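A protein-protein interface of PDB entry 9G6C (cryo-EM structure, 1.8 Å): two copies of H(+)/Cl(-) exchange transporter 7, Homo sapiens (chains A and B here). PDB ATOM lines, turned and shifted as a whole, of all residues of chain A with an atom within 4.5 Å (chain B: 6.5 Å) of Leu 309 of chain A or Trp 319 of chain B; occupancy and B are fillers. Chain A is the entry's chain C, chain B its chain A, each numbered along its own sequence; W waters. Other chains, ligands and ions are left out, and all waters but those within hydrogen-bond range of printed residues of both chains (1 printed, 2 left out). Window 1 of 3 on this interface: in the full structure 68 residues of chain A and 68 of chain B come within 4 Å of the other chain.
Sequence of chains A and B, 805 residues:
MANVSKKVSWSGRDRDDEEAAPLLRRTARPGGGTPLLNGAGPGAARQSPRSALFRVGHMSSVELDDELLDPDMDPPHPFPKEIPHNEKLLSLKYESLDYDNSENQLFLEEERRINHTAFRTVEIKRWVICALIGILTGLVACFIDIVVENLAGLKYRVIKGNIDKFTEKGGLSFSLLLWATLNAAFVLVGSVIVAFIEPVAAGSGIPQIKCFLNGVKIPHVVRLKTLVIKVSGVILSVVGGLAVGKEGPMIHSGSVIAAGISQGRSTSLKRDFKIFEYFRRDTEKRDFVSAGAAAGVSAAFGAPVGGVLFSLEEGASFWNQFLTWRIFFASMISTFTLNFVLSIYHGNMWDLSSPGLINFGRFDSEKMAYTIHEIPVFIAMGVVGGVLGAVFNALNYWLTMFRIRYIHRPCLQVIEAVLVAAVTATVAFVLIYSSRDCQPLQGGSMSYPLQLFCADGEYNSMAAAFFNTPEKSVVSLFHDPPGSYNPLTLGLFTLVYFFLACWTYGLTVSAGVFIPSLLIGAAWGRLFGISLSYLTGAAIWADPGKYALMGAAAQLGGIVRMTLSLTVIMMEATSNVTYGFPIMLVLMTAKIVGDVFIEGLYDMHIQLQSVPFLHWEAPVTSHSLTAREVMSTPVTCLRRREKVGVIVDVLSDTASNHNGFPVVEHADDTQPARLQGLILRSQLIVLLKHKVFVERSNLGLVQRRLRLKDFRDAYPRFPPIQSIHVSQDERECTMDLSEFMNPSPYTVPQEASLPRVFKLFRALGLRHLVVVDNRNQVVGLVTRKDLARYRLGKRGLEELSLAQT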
ATOM      1  N   VAL A 305      30.230   1.843  -0.347  1.00  0.00           N
ATOM      2  CA  VAL A 305      28.835   1.491  -0.107  1.00  0.00           C
ATOM      3  C   VAL A 305      28.000   2.747   0.099  1.00  0.00           C
ATOM      4  O   VAL A 305      26.853   2.828  -0.359  1.00  0.00           O
ATOM      5  CB  VAL A 305      28.718   0.525   1.085  1.00  0.00           C
ATOM      6  CG1 VAL A 305      27.281   0.067   1.252  1.00  0.00           C
ATOM      7  CG2 VAL A 305      29.634  -0.667   0.887  1.00  0.00           C
ATOM      8  N   GLY A 306      28.557   3.743   0.789  1.00  0.00           N
ATOM      9  CA  GLY A 306      27.867   5.013   0.927  1.00  0.00           C
ATOM     10  C   GLY A 306      27.625   5.696  -0.403  1.00  0.00           C
ATOM     11  O   GLY A 306      26.612   6.376  -0.582  1.00  0.00           O
ATOM     12  N   GLY A 307      28.551   5.532  -1.351  1.00  0.00           N
ATOM     13  CA  GLY A 307      28.330   6.065  -2.684  1.00  0.00           C
ATOM     14  C   GLY A 307      27.174   5.393  -3.396  1.00  0.00           C
ATOM     15  O   GLY A 307      26.381   6.051  -4.073  1.00  0.00           O
ATOM     16  N   VAL A 308      27.062   4.070  -3.251  1.00  0.00           N
ATOM     17  CA  VAL A 308      25.968   3.339  -3.884  1.00  0.00           C
ATOM     18  C   VAL A 308      24.629   3.808  -3.333  1.00  0.00           C
ATOM     19  O   VAL A 308      23.679   4.058  -4.084  1.00  0.00           O
ATOM     20  CB  VAL A 308      26.154   1.825  -3.687  1.00  0.00           C
ATOM     21  CG1 VAL A 308      24.958   1.063  -4.241  1.00  0.00           C
ATOM     22  CG2 VAL A 308      27.439   1.364  -4.341  1.00  0.00           C
ATOM     23  N   LEU A 309      24.538   3.946  -2.010  1.00  0.00           N
ATOM     24  CA  LEU A 309      23.277   4.343  -1.395  1.00  0.00           C
ATOM     25  C   LEU A 309      22.925   5.789  -1.711  1.00  0.00           C
ATOM     26  O   LEU A 309      21.742   6.143  -1.738  1.00  0.00           O
ATOM     27  CB  LEU A 309      23.338   4.118   0.113  1.00  0.00           C
ATOM     28  CG  LEU A 309      23.173   2.652   0.514  1.00  0.00           C
ATOM     29  CD1 LEU A 309      23.739   2.405   1.896  1.00  0.00           C
ATOM     30  CD2 LEU A 309      21.713   2.236   0.445  1.00  0.00           C
ATOM     31  N   PHE A 310      23.928   6.638  -1.943  1.00  0.00           N
ATOM     32  CA  PHE A 310      23.650   8.003  -2.377  1.00  0.00           C
ATOM     33  C   PHE A 310      22.970   8.011  -3.741  1.00  0.00           C
ATOM     34  O   PHE A 310      21.956   8.689  -3.939  1.00  0.00           O
ATOM     35  CB  PHE A 310      24.943   8.819  -2.408  1.00  0.00           C
ATOM     36  CG  PHE A 310      24.785  10.182  -3.021  1.00  0.00           C
ATOM     37  CD1 PHE A 310      24.317  11.243  -2.266  1.00  0.00           C
ATOM     38  CD2 PHE A 310      25.111  10.402  -4.349  1.00  0.00           C
ATOM     39  CE1 PHE A 310      24.169  12.498  -2.824  1.00  0.00           C
ATOM     40  CE2 PHE A 310      24.965  11.654  -4.913  1.00  0.00           C
ATOM     41  CZ  PHE A 310      24.496  12.704  -4.150  1.00  0.00           C
ATOM     42  N   SER A 311      23.516   7.255  -4.695  1.00  0.00           N
ATOM     43  CA  SER A 311      22.914   7.197  -6.024  1.00  0.00           C
ATOM     44  C   SER A 311      21.563   6.495  -5.988  1.00  0.00           C
ATOM     45  O   SER A 311      20.639   6.879  -6.715  1.00  0.00           O
ATOM     46  CB  SER A 311      23.861   6.498  -6.999  1.00  0.00           C
ATOM     47  OG  SER A 311      23.972   5.118  -6.699  1.00  0.00           O
ATOM     48  N   LEU A 312      21.429   5.461  -5.154  1.00  0.00           N
ATOM     49  CA  LEU A 312      20.144   4.786  -5.013  1.00  0.00           C
ATOM     50  C   LEU A 312      19.093   5.717  -4.420  1.00  0.00           C
ATOM     51  O   LEU A 312      17.930   5.697  -4.838  1.00  0.00           O
ATOM     52  CB  LEU A 312      20.298   3.530  -4.154  1.00  0.00           C
ATOM     53  CG  LEU A 312      21.041   2.356  -4.791  1.00  0.00           C
ATOM     54  CD1 LEU A 312      21.173   1.204  -3.808  1.00  0.00           C
ATOM     55  CD2 LEU A 312      20.342   1.904  -6.063  1.00  0.00           C
ATOM     56  N   GLU A 313      19.482   6.530  -3.436  1.00  0.00           N
ATOM     57  CA  GLU A 313      18.551   7.488  -2.849  1.00  0.00           C
ATOM     58  C   GLU A 313      18.102   8.521  -3.875  1.00  0.00           C
ATOM     59  O   GLU A 313      16.916   8.857  -3.958  1.00  0.00           O
ATOM     60  CB  GLU A 313      19.195   8.182  -1.650  1.00  0.00           C
ATOM     61  CG  GLU A 313      19.140   7.397  -0.358  1.00  0.00           C
ATOM     62  CD  GLU A 313      19.715   8.177   0.805  1.00  0.00           C
ATOM     63  OE1 GLU A 313      20.656   8.968   0.583  1.00  0.00           O
ATOM     64  OE2 GLU A 313      19.217   8.014   1.937  1.00  0.00           O
ATOM     65  N   ALA A 316      16.038   6.785  -6.801  1.00  0.00           N
ATOM     66  CA  ALA A 316      14.744   6.394  -6.238  1.00  0.00           C
ATOM     67  C   ALA A 316      13.911   5.613  -7.250  1.00  0.00           C
ATOM     68  O   ALA A 316      12.701   5.806  -7.375  1.00  0.00           O
ATOM     69  CB  ALA A 316      13.976   7.612  -5.722  1.00  0.00           C
ATOM     70  N   SER A 317      14.569   4.722  -7.982  1.00  0.00           N
ATOM     71  CA  SER A 317      13.935   3.986  -9.060  1.00  0.00           C
ATOM     72  C   SER A 317      13.599   2.565  -8.615  1.00  0.00           C
ATOM     73  O   SER A 317      13.782   2.183  -7.457  1.00  0.00           O
ATOM     74  CB  SER A 317      14.836   3.975 -10.297  1.00  0.00           C
ATOM     75  OG  SER A 317      15.865   3.010 -10.169  1.00  0.00           O
ATOM     76  N   LEU A 564      20.470   8.113   5.391  1.00  0.00           N
ATOM     77  CA  LEU A 564      20.856   6.727   5.140  1.00  0.00           C
ATOM     78  C   LEU A 564      22.228   6.637   4.483  1.00  0.00           C
ATOM     79  O   LEU A 564      23.089   5.872   4.931  1.00  0.00           O
ATOM     80  CB  LEU A 564      19.801   6.030   4.281  1.00  0.00           C
ATOM     81  CG  LEU A 564      20.158   4.627   3.785  1.00  0.00           C
ATOM     82  CD1 LEU A 564      20.041   3.614   4.911  1.00  0.00           C
ATOM     83  CD2 LEU A 564      19.276   4.233   2.611  1.00  0.00           C
ATOM     84  N   SER A 565      22.445   7.403   3.413  1.00  0.00           N
ATOM     85  CA  SER A 565      23.764   7.430   2.791  1.00  0.00           C
ATOM     86  C   SER A 565      24.804   8.003   3.743  1.00  0.00           C
ATOM     87  O   SER A 565      25.932   7.502   3.819  1.00  0.00           O
ATOM     88  CB  SER A 565      23.719   8.234   1.493  1.00  0.00           C
ATOM     89  OG  SER A 565      23.001   9.442   1.668  1.00  0.00           O
ATOM     90  N   VAL A 568      25.925   5.437   6.487  1.00  0.00           N
ATOM     91  CA  VAL A 568      26.827   4.421   5.958  1.00  0.00           C
ATOM     92  C   VAL A 568      28.180   5.032   5.617  1.00  0.00           C
ATOM     93  O   VAL A 568      29.228   4.405   5.812  1.00  0.00           O
ATOM     94  CB  VAL A 568      26.183   3.726   4.745  1.00  0.00           C
ATOM     95  CG1 VAL A 568      27.180   2.806   4.058  1.00  0.00           C
ATOM     96  CG2 VAL A 568      24.953   2.953   5.188  1.00  0.00           C
ATOM     97  N   TRP A 616      10.650  11.961  -2.535  1.00  0.00           N
ATOM     98  CA  TRP A 616      10.487  10.512  -2.508  1.00  0.00           C
ATOM     99  C   TRP A 616       9.020  10.112  -2.589  1.00  0.00           C
ATOM    100  O   TRP A 616       8.692   9.042  -3.116  1.00  0.00           O
ATOM    101  CB  TRP A 616      11.135   9.935  -1.250  1.00  0.00           C
ATOM    102  CG  TRP A 616      12.629   9.912  -1.310  1.00  0.00           C
ATOM    103  CD1 TRP A 616      13.401   9.278  -2.239  1.00  0.00           C
ATOM    104  CD2 TRP A 616      13.536  10.548  -0.401  1.00  0.00           C
ATOM    105  NE1 TRP A 616      14.732   9.480  -1.966  1.00  0.00           N
ATOM    106  CE2 TRP A 616      14.841  10.256  -0.843  1.00  0.00           C
ATOM    107  CE3 TRP A 616      13.369  11.336   0.742  1.00  0.00           C
ATOM    108  CZ2 TRP A 616      15.974  10.724  -0.182  1.00  0.00           C
ATOM    109  CZ3 TRP A 616      14.496  11.799   1.396  1.00  0.00           C
ATOM    110  CH2 TRP A 616      15.781  11.492   0.933  1.00  0.00           C
ATOM    111  N   VAL B 305      24.539  -2.967   7.232  1.00  0.00           N
ATOM    112  CA  VAL B 305      24.340  -2.527   5.856  1.00  0.00           C
ATOM    113  C   VAL B 305      24.176  -3.728   4.936  1.00  0.00           C
ATOM    114  O   VAL B 305      23.377  -3.701   3.992  1.00  0.00           O
ATOM    115  CB  VAL B 305      25.496  -1.615   5.407  1.00  0.00           C
ATOM    116  CG1 VAL B 305      25.208  -1.041   4.031  1.00  0.00           C
ATOM    117  CG2 VAL B 305      25.708  -0.499   6.414  1.00  0.00           C
ATOM    118  N   VAL B 308      20.611  -4.788   5.107  1.00  0.00           N
ATOM    119  CA  VAL B 308      19.718  -3.939   4.323  1.00  0.00           C
ATOM    120  C   VAL B 308      19.762  -4.341   2.855  1.00  0.00           C
ATOM    121  O   VAL B 308      18.725  -4.477   2.197  1.00  0.00           O
ATOM    122  CB  VAL B 308      20.088  -2.457   4.509  1.00  0.00           C
ATOM    123  CG1 VAL B 308      19.253  -1.579   3.589  1.00  0.00           C
ATOM    124  CG2 VAL B 308      19.911  -2.050   5.955  1.00  0.00           C
ATOM    125  N   LEU B 309      20.968  -4.548   2.324  1.00  0.00           N
ATOM    126  CA  LEU B 309      21.103  -4.883   0.912  1.00  0.00           C
ATOM    127  C   LEU B 309      20.577  -6.279   0.610  1.00  0.00           C
ATOM    128  O   LEU B 309      20.140  -6.541  -0.517  1.00  0.00           O
ATOM    129  CB  LEU B 309      22.561  -4.751   0.481  1.00  0.00           C
ATOM    130  CG  LEU B 309      23.010  -3.299   0.303  1.00  0.00           C
ATOM    131  CD1 LEU B 309      24.520  -3.204   0.266  1.00  0.00           C
ATOM    132  CD2 LEU B 309      22.398  -2.696  -0.951  1.00  0.00           C
ATOM    133  N   LEU B 312      16.870  -5.644   0.349  1.00  0.00           N
ATOM    134  CA  LEU B 312      16.636  -4.886  -0.875  1.00  0.00           C
ATOM    135  C   LEU B 312      16.784  -5.770  -2.107  1.00  0.00           C
ATOM    136  O   LEU B 312      16.016  -5.640  -3.067  1.00  0.00           O
ATOM    137  CB  LEU B 312      17.593  -3.695  -0.949  1.00  0.00           C
ATOM    138  CG  LEU B 312      17.331  -2.550   0.031  1.00  0.00           C
ATOM    139  CD1 LEU B 312      18.405  -1.480  -0.092  1.00  0.00           C
ATOM    140  CD2 LEU B 312      15.950  -1.957  -0.190  1.00  0.00           C
ATOM    141  N   SER B 317      12.029  -4.234  -5.128  1.00  0.00           N
ATOM    142  CA  SER B 317      10.863  -3.392  -5.330  1.00  0.00           C
ATOM    143  C   SER B 317      11.283  -1.977  -5.716  1.00  0.00           C
ATOM    144  O   SER B 317      12.464  -1.675  -5.907  1.00  0.00           O
ATOM    145  CB  SER B 317       9.992  -3.382  -4.072  1.00  0.00           C
ATOM    146  OG  SER B 317      10.536  -2.526  -3.084  1.00  0.00           O
ATOM    147  N   PHE B 318      10.289  -1.103  -5.849  1.00  0.00           N
ATOM    148  CA  PHE B 318      10.563   0.313  -6.038  1.00  0.00           C
ATOM    149  C   PHE B 318      11.266   0.865  -4.807  1.00  0.00           C
ATOM    150  O   PHE B 318      11.007   0.433  -3.680  1.00  0.00           O
ATOM    151  CB  PHE B 318       9.263   1.081  -6.290  1.00  0.00           C
ATOM    152  CG  PHE B 318       8.265   0.967  -5.170  1.00  0.00           C
ATOM    153  CD1 PHE B 318       7.384  -0.101  -5.111  1.00  0.00           C
ATOM    154  CD2 PHE B 318       8.213   1.927  -4.172  1.00  0.00           C
ATOM    155  CE1 PHE B 318       6.470  -0.207  -4.080  1.00  0.00           C
ATOM    156  CE2 PHE B 318       7.302   1.826  -3.139  1.00  0.00           C
ATOM    157  CZ  PHE B 318       6.429   0.758  -3.092  1.00  0.00           C
ATOM    158  N   TRP B 319      12.169   1.817  -5.023  1.00  0.00           N
ATOM    159  CA  TRP B 319      12.904   2.396  -3.908  1.00  0.00           C
ATOM    160  C   TRP B 319      11.949   3.081  -2.941  1.00  0.00           C
ATOM    161  O   TRP B 319      11.204   3.988  -3.322  1.00  0.00           O
ATOM    162  CB  TRP B 319      13.950   3.386  -4.413  1.00  0.00           C
ATOM    163  CG  TRP B 319      14.759   3.981  -3.306  1.00  0.00           C
ATOM    164  CD1 TRP B 319      14.563   5.190  -2.705  1.00  0.00           C
ATOM    165  CD2 TRP B 319      15.879   3.381  -2.646  1.00  0.00           C
ATOM    166  NE1 TRP B 319      15.500   5.385  -1.720  1.00  0.00           N
ATOM    167  CE2 TRP B 319      16.318   4.290  -1.663  1.00  0.00           C
ATOM    168  CE3 TRP B 319      16.555   2.167  -2.796  1.00  0.00           C
ATOM    169  CZ2 TRP B 319      17.404   4.021  -0.833  1.00  0.00           C
ATOM    170  CZ3 TRP B 319      17.632   1.903  -1.972  1.00  0.00           C
ATOM    171  CH2 TRP B 319      18.046   2.827  -1.003  1.00  0.00           C
ATOM    172  N   ASN B 320      11.973   2.640  -1.687  1.00  0.00           N
ATOM    173  CA  ASN B 320      11.151   3.201  -0.621  1.00  0.00           C
ATOM    174  C   ASN B 320      12.117   3.741   0.429  1.00  0.00           C
ATOM    175  O   ASN B 320      12.680   2.975   1.215  1.00  0.00           O
ATOM    176  CB  ASN B 320      10.206   2.150  -0.044  1.00  0.00           C
ATOM    177  CG  ASN B 320       9.152   2.746   0.872  1.00  0.00           C
ATOM    178  OD1 ASN B 320       9.318   3.842   1.404  1.00  0.00           O
ATOM    179  ND2 ASN B 320       8.058   2.018   1.060  1.00  0.00           N
ATOM    180  N   GLN B 321      12.310   5.062   0.426  1.00  0.00           N
ATOM    181  CA  GLN B 321      13.315   5.671   1.292  1.00  0.00           C
ATOM    182  C   GLN B 321      12.989   5.449   2.763  1.00  0.00           C
ATOM    183  O   GLN B 321      13.871   5.117   3.563  1.00  0.00           O
ATOM    184  CB  GLN B 321      13.426   7.166   0.985  1.00  0.00           C
ATOM    185  CG  GLN B 321      14.424   7.907   1.856  1.00  0.00           C
ATOM    186  CD  GLN B 321      15.859   7.626   1.462  1.00  0.00           C
ATOM    187  OE1 GLN B 321      16.121   6.969   0.455  1.00  0.00           O
ATOM    188  NE2 GLN B 321      16.800   8.122   2.257  1.00  0.00           N
ATOM    189  N   PHE B 322      11.722   5.626   3.140  1.00  0.00           N
ATOM    190  CA  PHE B 322      11.346   5.499   4.544  1.00  0.00           C
ATOM    191  C   PHE B 322      11.378   4.046   4.999  1.00  0.00           C
ATOM    192  O   PHE B 322      11.714   3.761   6.154  1.00  0.00           O
ATOM    193  CB  PHE B 322       9.967   6.116   4.775  1.00  0.00           C
ATOM    194  CG  PHE B 322       9.821   7.499   4.205  1.00  0.00           C
ATOM    195  CD1 PHE B 322       9.440   7.687   2.885  1.00  0.00           C
ATOM    196  CD2 PHE B 322      10.079   8.612   4.987  1.00  0.00           C
ATOM    197  CE1 PHE B 322       9.313   8.958   2.360  1.00  0.00           C
ATOM    198  CE2 PHE B 322       9.954   9.886   4.468  1.00  0.00           C
ATOM    199  CZ  PHE B 322       9.569  10.059   3.154  1.00  0.00           C
ATOM    200  N   THR B 324      13.455   1.713   3.672  1.00  0.00           N
ATOM    201  CA  THR B 324      14.873   1.380   3.762  1.00  0.00           C
ATOM    202  C   THR B 324      15.500   1.984   5.010  1.00  0.00           C
ATOM    203  O   THR B 324      16.367   1.368   5.642  1.00  0.00           O
ATOM    204  CB  THR B 324      15.606   1.859   2.509  1.00  0.00           C
ATOM    205  OG1 THR B 324      14.871   1.466   1.344  1.00  0.00           O
ATOM    206  CG2 THR B 324      17.001   1.257   2.445  1.00  0.00           C
HETATM  207  O   HOH W   1      10.764   5.226  -5.949  1.00  0.00           O
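The backbone NH (N) of Trp 319 of chain B lies within hydrogen-bond range of the backbone carbonyl oxygen (O) of Ser 317 of chain A, 2.9 Å away. NE2 of Gln 321 of chain B is in hydrogen-bond range of OE2 of Glu 313 of chain A.
NE1 of Trp 319 of chain B sits at hydrogen-bond distance from OE1 of Gln 321 of chain B (2.8 Å). The backbone carbonyl oxygen (O) of Asn 320 of chain B lies within hydrogen-bond range of the side-chain hydroxyl (OG1) of Thr 324 of chain B (2.7 Å). OE1 of Glu 313 of chain A is in hydrogen-bond range of OG of Ser 565 of chain A. The backbone carbonyl oxygen (O) of Glu 313 of chain A sits at hydrogen-bond distance from the indole nitrogen (NE1) of Trp 616 of chain A, at 3.0 Å.
Among the printed residues, pairs that only touch across the chains: Trp 616 of chain A with Gln 321 of chain B (3.5 Å), Ala 316 of chain A with Trp 319 of chain B (3.6 Å), Val 305 of chain A with Val 305 of chain B (3.6 Å), Val 568 of chain A with Val 305 of chain B (3.7 Å), Leu 564 of chain A with Thr 324 of chain B (3.7 Å), Leu 312 of chain A with Trp 319 of chain B (3.8 Å), Glu 313 of chain A with Trp 319 of chain B (3.8 Å), Ser 317 of chain A with Phe 318 of chain B (3.9 Å), Leu 564 of chain A with Trp 319 of chain B (3.9 Å) and Leu 309 of chain A with Trp 319 of chain B (3.99 Å).
Of the printed residues of chain B, Val 305 of chain A touches Val 305 (3.6 Å). Of the printed residues of chain B, Leu 309 of chain A touches Trp 319 (3.99 Å). Of the printed residues of chain B, Leu 312 of chain A touches Trp 319 (3.8 Å). Printed residues of chain B within 4 Å of Glu 313 of chain A: Trp 319 (3.8 Å) and Gln 321 (2.4 Å). Of the printed residues of chain A, Trp 319 of chain B touches Leu 309 (3.99 Å), Leu 312 (3.8 Å), Glu 313 (3.8 Å), Ala 316 (3.6 Å), Ser 317 (2.9 Å) and Leu 564 (3.9 Å). Printed residues of chain A within 4 Å of Gln 321 of chain B: Glu 313 (2.4 Å) and Trp 616 (3.5 Å). Printed residues of chain A within 4 Å of Thr 324 of chain B: Leu 564.
Hydrophobic or aromatic side chains of chain B that line the printed part of chain A: Val 305 and Trp 319. Printed residues of chain A that touch a printed residue of chain B: Val 305, Leu 309, Leu 312, Glu 313, Ala 316, Ser 317, Leu 564, Val 568 and Trp 616. Hydrophobic or aromatic side chains of chain A that line the printed part of chain B: Val 305, Leu 309, Leu 312, Ala 316, Leu 564, Val 568 and Trp 616. Among the printed residues, 12 pairs touch across the chains.
Val 305 of chain A touches its own counterpart, Val 305 of chain B.
Water W1 bridges O of Ala 316 of chain A and O of Trp 319 of chain B.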
